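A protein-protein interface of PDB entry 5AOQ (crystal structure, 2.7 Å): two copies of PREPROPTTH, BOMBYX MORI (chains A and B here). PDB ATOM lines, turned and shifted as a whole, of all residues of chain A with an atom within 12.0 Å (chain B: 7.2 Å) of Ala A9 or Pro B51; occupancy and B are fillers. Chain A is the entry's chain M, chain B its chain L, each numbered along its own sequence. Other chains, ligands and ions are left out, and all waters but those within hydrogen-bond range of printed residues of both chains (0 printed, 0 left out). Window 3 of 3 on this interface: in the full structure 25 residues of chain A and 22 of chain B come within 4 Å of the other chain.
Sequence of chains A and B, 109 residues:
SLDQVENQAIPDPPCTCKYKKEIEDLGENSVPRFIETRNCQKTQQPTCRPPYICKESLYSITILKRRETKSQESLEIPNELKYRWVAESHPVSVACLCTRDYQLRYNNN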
ATOM      1  N   ALA A   9      18.424   3.645  19.467  1.00  0.00           N
ATOM      2  CA  ALA A   9      18.199   3.647  20.908  1.00  0.00           C
ATOM      3  C   ALA A   9      18.534   2.288  21.509  1.00  0.00           C
ATOM      4  O   ALA A   9      19.298   2.195  22.470  1.00  0.00           O
ATOM      5  CB  ALA A   9      16.759   4.024  21.220  1.00  0.00           C
ATOM      6  N   ILE A  10      17.959   1.238  20.930  1.00  0.00           N
ATOM      7  CA  ILE A  10      18.145  -0.125  21.421  1.00  0.00           C
ATOM      8  C   ILE A  10      19.096  -0.909  20.514  1.00  0.00           C
ATOM      9  O   ILE A  10      18.946  -0.880  19.293  1.00  0.00           O
ATOM     10  CB  ILE A  10      16.801  -0.879  21.502  1.00  0.00           C
ATOM     11  CG1 ILE A  10      15.769  -0.068  22.294  1.00  0.00           C
ATOM     12  CG2 ILE A  10      16.994  -2.257  22.122  1.00  0.00           C
ATOM     13  CD1 ILE A  10      16.175   0.244  23.722  1.00  0.00           C
ATOM     14  N   PRO A  11      20.079  -1.612  21.106  1.00  0.00           N
ATOM     15  CA  PRO A  11      20.970  -2.462  20.308  1.00  0.00           C
ATOM     16  C   PRO A  11      20.448  -3.888  20.149  1.00  0.00           C
ATOM     17  O   PRO A  11      19.592  -4.323  20.919  1.00  0.00           O
ATOM     18  CB  PRO A  11      22.267  -2.445  21.113  1.00  0.00           C
ATOM     19  CG  PRO A  11      21.808  -2.340  22.521  1.00  0.00           C
ATOM     20  CD  PRO A  11      20.541  -1.514  22.503  1.00  0.00           C
ATOM     21  N   ASP A  12      20.970  -4.603  19.156  1.00  0.00           N
ATOM     22  CA  ASP A  12      20.583  -5.987  18.908  1.00  0.00           C
ATOM     23  C   ASP A  12      21.692  -6.704  18.133  1.00  0.00           C
ATOM     24  O   ASP A  12      22.283  -6.118  17.229  1.00  0.00           O
ATOM     25  CB  ASP A  12      19.265  -6.046  18.130  1.00  0.00           C
ATOM     26  CG  ASP A  12      18.734  -7.460  17.988  1.00  0.00           C
ATOM     27  OD1 ASP A  12      18.028  -7.925  18.907  1.00  0.00           O
ATOM     28  OD2 ASP A  12      19.019  -8.102  16.957  1.00  0.00           O
ATOM     29  N   PRO A  13      21.996  -7.968  18.487  1.00  0.00           N
ATOM     30  CA  PRO A  13      21.455  -8.772  19.591  1.00  0.00           C
ATOM     31  C   PRO A  13      21.806  -8.191  20.958  1.00  0.00           C
ATOM     32  O   PRO A  13      22.826  -7.512  21.083  1.00  0.00           O
ATOM     33  CB  PRO A  13      22.120 -10.140  19.395  1.00  0.00           C
ATOM     34  CG  PRO A  13      22.549 -10.164  17.974  1.00  0.00           C
ATOM     35  CD  PRO A  13      22.917  -8.755  17.650  1.00  0.00           C
ATOM     36  N   PRO A  14      20.973  -8.457  21.975  1.00  0.00           N
ATOM     37  CA  PRO A  14      21.168  -7.828  23.284  1.00  0.00           C
ATOM     38  C   PRO A  14      22.347  -8.404  24.066  1.00  0.00           C
ATOM     39  O   PRO A  14      22.874  -9.457  23.710  1.00  0.00           O
ATOM     40  CB  PRO A  14      19.846  -8.110  24.001  1.00  0.00           C
ATOM     41  CG  PRO A  14      19.367  -9.384  23.404  1.00  0.00           C
ATOM     42  CD  PRO A  14      19.814  -9.368  21.967  1.00  0.00           C
ATOM     43  N   CYS A  15      22.747  -7.706  25.123  1.00  0.00           N
ATOM     44  CA  CYS A  15      23.881  -8.119  25.942  1.00  0.00           C
ATOM     45  C   CYS A  15      23.601  -9.440  26.647  1.00  0.00           C
ATOM     46  O   CYS A  15      24.489 -10.282  26.779  1.00  0.00           O
ATOM     47  CB  CYS A  15      24.207  -7.046  26.979  1.00  0.00           C
ATOM     48  SG  CYS A  15      23.218  -7.179  28.487  1.00  0.00           S
ATOM     49  N   THR A  16      22.362  -9.604  27.106  1.00  0.00           N
ATOM     50  CA  THR A  16      21.958 -10.791  27.852  1.00  0.00           C
ATOM     51  C   THR A  16      22.270 -12.071  27.089  1.00  0.00           C
ATOM     52  O   THR A  16      22.118 -12.129  25.868  1.00  0.00           O
ATOM     53  CB  THR A  16      20.448 -10.764  28.178  1.00  0.00           C
ATOM     54  OG1 THR A  16      20.086 -11.964  28.871  1.00  0.00           O
ATOM     55  CG2 THR A  16      19.617 -10.646  26.904  1.00  0.00           C
ATOM     56  N   CYS B  48      24.758  -2.578  34.249  1.00  0.00           N
ATOM     57  CA  CYS B  48      23.768  -2.909  33.229  1.00  0.00           C
ATOM     58  C   CYS B  48      22.747  -1.778  33.116  1.00  0.00           C
ATOM     59  O   CYS B  48      21.536  -1.998  33.169  1.00  0.00           O
ATOM     60  CB  CYS B  48      23.068  -4.235  33.546  1.00  0.00           C
ATOM     61  SG  CYS B  48      22.071  -4.864  32.173  1.00  0.00           S
ATOM     62  N   ARG B  49      23.266  -0.560  32.983  1.00  0.00           N
ATOM     63  CA  ARG B  49      22.465   0.652  32.830  1.00  0.00           C
ATOM     64  C   ARG B  49      21.520   0.537  31.633  1.00  0.00           C
ATOM     65  O   ARG B  49      21.658  -0.389  30.833  1.00  0.00           O
ATOM     66  CB  ARG B  49      23.388   1.866  32.676  1.00  0.00           C
ATOM     67  CG  ARG B  49      24.388   2.038  33.810  1.00  0.00           C
ATOM     68  CD  ARG B  49      23.713   2.008  35.176  1.00  0.00           C
ATOM     69  NE  ARG B  49      22.591   2.942  35.255  1.00  0.00           N
ATOM     70  CZ  ARG B  49      21.787   3.061  36.308  1.00  0.00           C
ATOM     71  NH1 ARG B  49      21.973   2.305  37.380  1.00  0.00           N
ATOM     72  NH2 ARG B  49      20.792   3.939  36.290  1.00  0.00           N
ATOM     73  N   PRO B  50      20.536   1.452  31.524  1.00  0.00           N
ATOM     74  CA  PRO B  50      19.586   1.396  30.404  1.00  0.00           C
ATOM     75  C   PRO B  50      20.269   1.246  29.039  1.00  0.00           C
ATOM     76  O   PRO B  50      21.458   1.547  28.924  1.00  0.00           O
ATOM     77  CB  PRO B  50      18.874   2.746  30.495  1.00  0.00           C
ATOM     78  CG  PRO B  50      18.890   3.073  31.934  1.00  0.00           C
ATOM     79  CD  PRO B  50      20.188   2.526  32.475  1.00  0.00           C
ATOM     80  N   PRO B  51      19.525   0.818  28.005  1.00  0.00           N
ATOM     81  CA  PRO B  51      18.079   0.561  27.980  1.00  0.00           C
ATOM     82  C   PRO B  51      17.661  -0.672  28.785  1.00  0.00           C
ATOM     83  O   PRO B  51      16.468  -0.859  29.027  1.00  0.00           O
ATOM     84  CB  PRO B  51      17.781   0.349  26.489  1.00  0.00           C
ATOM     85  CG  PRO B  51      18.993   0.846  25.759  1.00  0.00           C
ATOM     86  CD  PRO B  51      20.131   0.608  26.681  1.00  0.00           C
ATOM     87  N   TYR B  52      18.624  -1.497  29.190  1.00  0.00           N
ATOM     88  CA  TYR B  52      18.320  -2.688  29.976  1.00  0.00           C
ATOM     89  C   TYR B  52      18.104  -2.303  31.432  1.00  0.00           C
ATOM     90  O   TYR B  52      18.819  -1.452  31.955  1.00  0.00           O
ATOM     91  CB  TYR B  52      19.454  -3.710  29.896  1.00  0.00           C
ATOM     92  CG  TYR B  52      19.923  -4.044  28.502  1.00  0.00           C
ATOM     93  CD1 TYR B  52      20.905  -3.283  27.883  1.00  0.00           C
ATOM     94  CD2 TYR B  52      19.403  -5.129  27.813  1.00  0.00           C
ATOM     95  CE1 TYR B  52      21.345  -3.585  26.614  1.00  0.00           C
ATOM     96  CE2 TYR B  52      19.838  -5.440  26.541  1.00  0.00           C
ATOM     97  CZ  TYR B  52      20.811  -4.664  25.947  1.00  0.00           C
ATOM     98  OH  TYR B  52      21.253  -4.962  24.683  1.00  0.00           O
ATOM     99  N   ILE B  53      17.136  -2.938  32.087  1.00  0.00           N
ATOM    100  CA  ILE B  53      16.920  -2.734  33.517  1.00  0.00           C
ATOM    101  C   ILE B  53      16.743  -4.077  34.225  1.00  0.00           C
ATOM    102  O   ILE B  53      16.188  -5.021  33.662  1.00  0.00           O
ATOM    103  CB  ILE B  53      15.705  -1.813  33.766  1.00  0.00           C
ATOM    104  CG1 ILE B  53      15.989  -0.407  33.225  1.00  0.00           C
ATOM    105  CG2 ILE B  53      15.349  -1.738  35.248  1.00  0.00           C
ATOM    106  CD1 ILE B  53      17.154   0.326  33.907  1.00  0.00           C
ATOM    107  N   LYS B  55      15.374  -6.978  36.096  1.00  0.00           N
ATOM    108  CA  LYS B  55      14.102  -7.609  36.447  1.00  0.00           C
ATOM    109  C   LYS B  55      14.343  -8.870  37.280  1.00  0.00           C
ATOM    110  O   LYS B  55      15.458  -9.388  37.306  1.00  0.00           O
ATOM    111  CB  LYS B  55      13.305  -7.927  35.184  1.00  0.00           C
ATOM    112  CG  LYS B  55      13.003  -6.682  34.365  1.00  0.00           C
ATOM    113  CD  LYS B  55      12.318  -7.000  33.050  1.00  0.00           C
ATOM    114  CE  LYS B  55      12.122  -5.741  32.217  1.00  0.00           C
ATOM    115  NZ  LYS B  55      13.413  -5.062  31.897  1.00  0.00           N
ATOM    116  N   CYS B  98      18.739  -9.018  33.283  1.00  0.00           N
ATOM    117  CA  CYS B  98      18.820  -7.641  32.817  1.00  0.00           C
ATOM    118  C   CYS B  98      18.521  -7.586  31.325  1.00  0.00           C
ATOM    119  O   CYS B  98      19.249  -6.957  30.558  1.00  0.00           O
ATOM    120  CB  CYS B  98      20.198  -7.048  33.111  1.00  0.00           C
ATOM    121  SG  CYS B  98      20.256  -5.244  33.000  1.00  0.00           S
ATOM    122  N   THR B  99      17.449  -8.261  30.921  1.00  0.00           N
ATOM    123  CA  THR B  99      17.011  -8.249  29.532  1.00  0.00           C
ATOM    124  C   THR B  99      15.980  -7.142  29.319  1.00  0.00           C
ATOM    125  O   THR B  99      15.150  -6.870  30.187  1.00  0.00           O
ATOM    126  CB  THR B  99      16.418  -9.613  29.109  1.00  0.00           C
ATOM    127  OG1 THR B  99      16.085  -9.586  27.716  1.00  0.00           O
ATOM    128  CG2 THR B  99      15.176  -9.954  29.926  1.00  0.00           C
ATOM    129  N   ARG B 100      16.051  -6.505  28.156  1.00  0.00           N
ATOM    130  CA  ARG B 100      15.176  -5.386  27.816  1.00  0.00           C
ATOM    131  C   ARG B 100      13.793  -5.843  27.355  1.00  0.00           C
ATOM    132  O   ARG B 100      12.924  -5.019  27.068  1.00  0.00           O
ATOM    133  CB  ARG B 100      15.822  -4.540  26.718  1.00  0.00           C
ATOM    134  CG  ARG B 100      16.217  -5.357  25.500  1.00  0.00           C
ATOM    135  CD  ARG B 100      16.739  -4.507  24.364  1.00  0.00           C
ATOM    136  NE  ARG B 100      17.433  -5.331  23.379  1.00  0.00           N
ATOM    137  CZ  ARG B 100      16.832  -6.200  22.571  1.00  0.00           C
ATOM    138  NH1 ARG B 100      15.517  -6.365  22.623  1.00  0.00           N
ATOM    139  NH2 ARG B 100      17.547  -6.911  21.710  1.00  0.00           N
ATOM    140  N   ASP B 101      13.592  -7.156  27.283  1.00  0.00           N
ATOM    141  CA  ASP B 101      12.354  -7.717  26.751  1.00  0.00           C
ATOM    142  C   ASP B 101      11.218  -7.668  27.770  1.00  0.00           C
ATOM    143  O   ASP B 101      11.398  -8.038  28.931  1.00  0.00           O
ATOM    144  CB  ASP B 101      12.582  -9.160  26.297  1.00  0.00           C
ATOM    145  CG  ASP B 101      13.687  -9.278  25.264  1.00  0.00           C
ATOM    146  OD1 ASP B 101      13.410  -9.051  24.069  1.00  0.00           O
ATOM    147  OD2 ASP B 101      14.830  -9.600  25.647  1.00  0.00           O
ATOM    148  N   GLN B 103       8.841  -4.968  29.242  1.00  0.00           N
ATOM    149  CA  GLN B 103       8.958  -4.025  30.352  1.00  0.00           C
ATOM    150  C   GLN B 103       7.584  -3.515  30.774  1.00  0.00           C
ATOM    151  O   GLN B 103       7.013  -2.638  30.128  1.00  0.00           O
ATOM    152  CB  GLN B 103       9.859  -2.850  29.966  1.00  0.00           C
ATOM    153  CG  GLN B 103      11.279  -3.257  29.603  1.00  0.00           C
ATOM    154  CD  GLN B 103      12.218  -2.072  29.471  1.00  0.00           C
ATOM    155  OE1 GLN B 103      13.389  -2.153  29.841  1.00  0.00           O
ATOM    156  NE2 GLN B 103      11.712  -0.967  28.932  1.00  0.00           N
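OH of Tyr B52 lies within hydrogen-bond range of N of Cys A15 (3.2 Å).
The guanidinium group of Arg B100 lies within hydrogen-bond range of the backbone carbonyl oxygen of Pro A11 (3.4 Å).
OD1 of Asp A12 lies within salt-bridge range of NH2 of Arg B100 (3.0 Å).
The backbone carbonyl oxygen of Pro B51 lies close to the side-chain amide oxygen of Gln B103 (3.4 Å).
NZ of Lys B55 is in hydrogen-bond range of O of Thr B99 (3.0 Å).
OG1 of Thr B99 is in hydrogen-bond range of OD2 of Asp B101 (2.4 Å).
OD1 of Asp B101 lies within salt-bridge range of NH1 of Arg B100, 3.7 Å away.
SG of Cys B98 forms a disulfide with SG of Cys B48, at 2.0 Å.
Among the printed residues, merely in contact across the chains: Ala A9 with Pro B51 (3.6 Å), Ile A10 with Pro B51 (3.2 Å), Ile A10 with Arg B100 (3.2 Å), Pro A11 with Tyr B52 (3.4 Å), Pro A14 with Tyr B52 (3.2 Å), Pro A14 with Arg B100 (3.4 Å) and Thr A16 with Thr B99 (3.8 Å).
Of chain B, only Pro B51 comes within 4 Å of Ala A9.
Of chain A, only Ala A9 (3.6 Å) and Ile A10 (3.2 Å) come within 4 Å of Pro B51.
Of the printed residues of chain B, Pro A14 touches Tyr B52 and Arg B100.
Of the printed residues of chain A, Thr B99 touches Thr A16 (3.8 Å).
Of the printed residues of chain B, Ile A10 touches Pro B51 (3.2 Å) and Arg B100 (3.2 Å).
Printed residues of chain B within 4 Å of Asp A12: Arg B100.
Lys B55 touches none of the printed residues of chain A.
The nearest residue of chain A that does not touch Pro B51 is Pro A11 (4.3 Å).
Of the 12 printed residues of chain B, 4 touch a printed residue of chain A.
Printed residues of chain B that touch a printed residue of chain A: Pro B51, Tyr B52, Thr B99 and Arg B100.
Hydrophobic or aromatic side chains of chain B within 4 Å of the printed part of chain A: Pro B51 and Tyr B52.
Of the 8 printed residues of chain A, 7 touch a printed residue of chain B.
Hydrophobic or aromatic side chains of chain A that line the printed part of chain B: Ile A10, Pro A11 and Pro A14.
Among the printed residues, 10 pairs touch across the chains.
No position is printed for both chains.
Of the 10 pairs that touch across the chains among the printed residues, none has its exchanged pair printed and touching as well.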
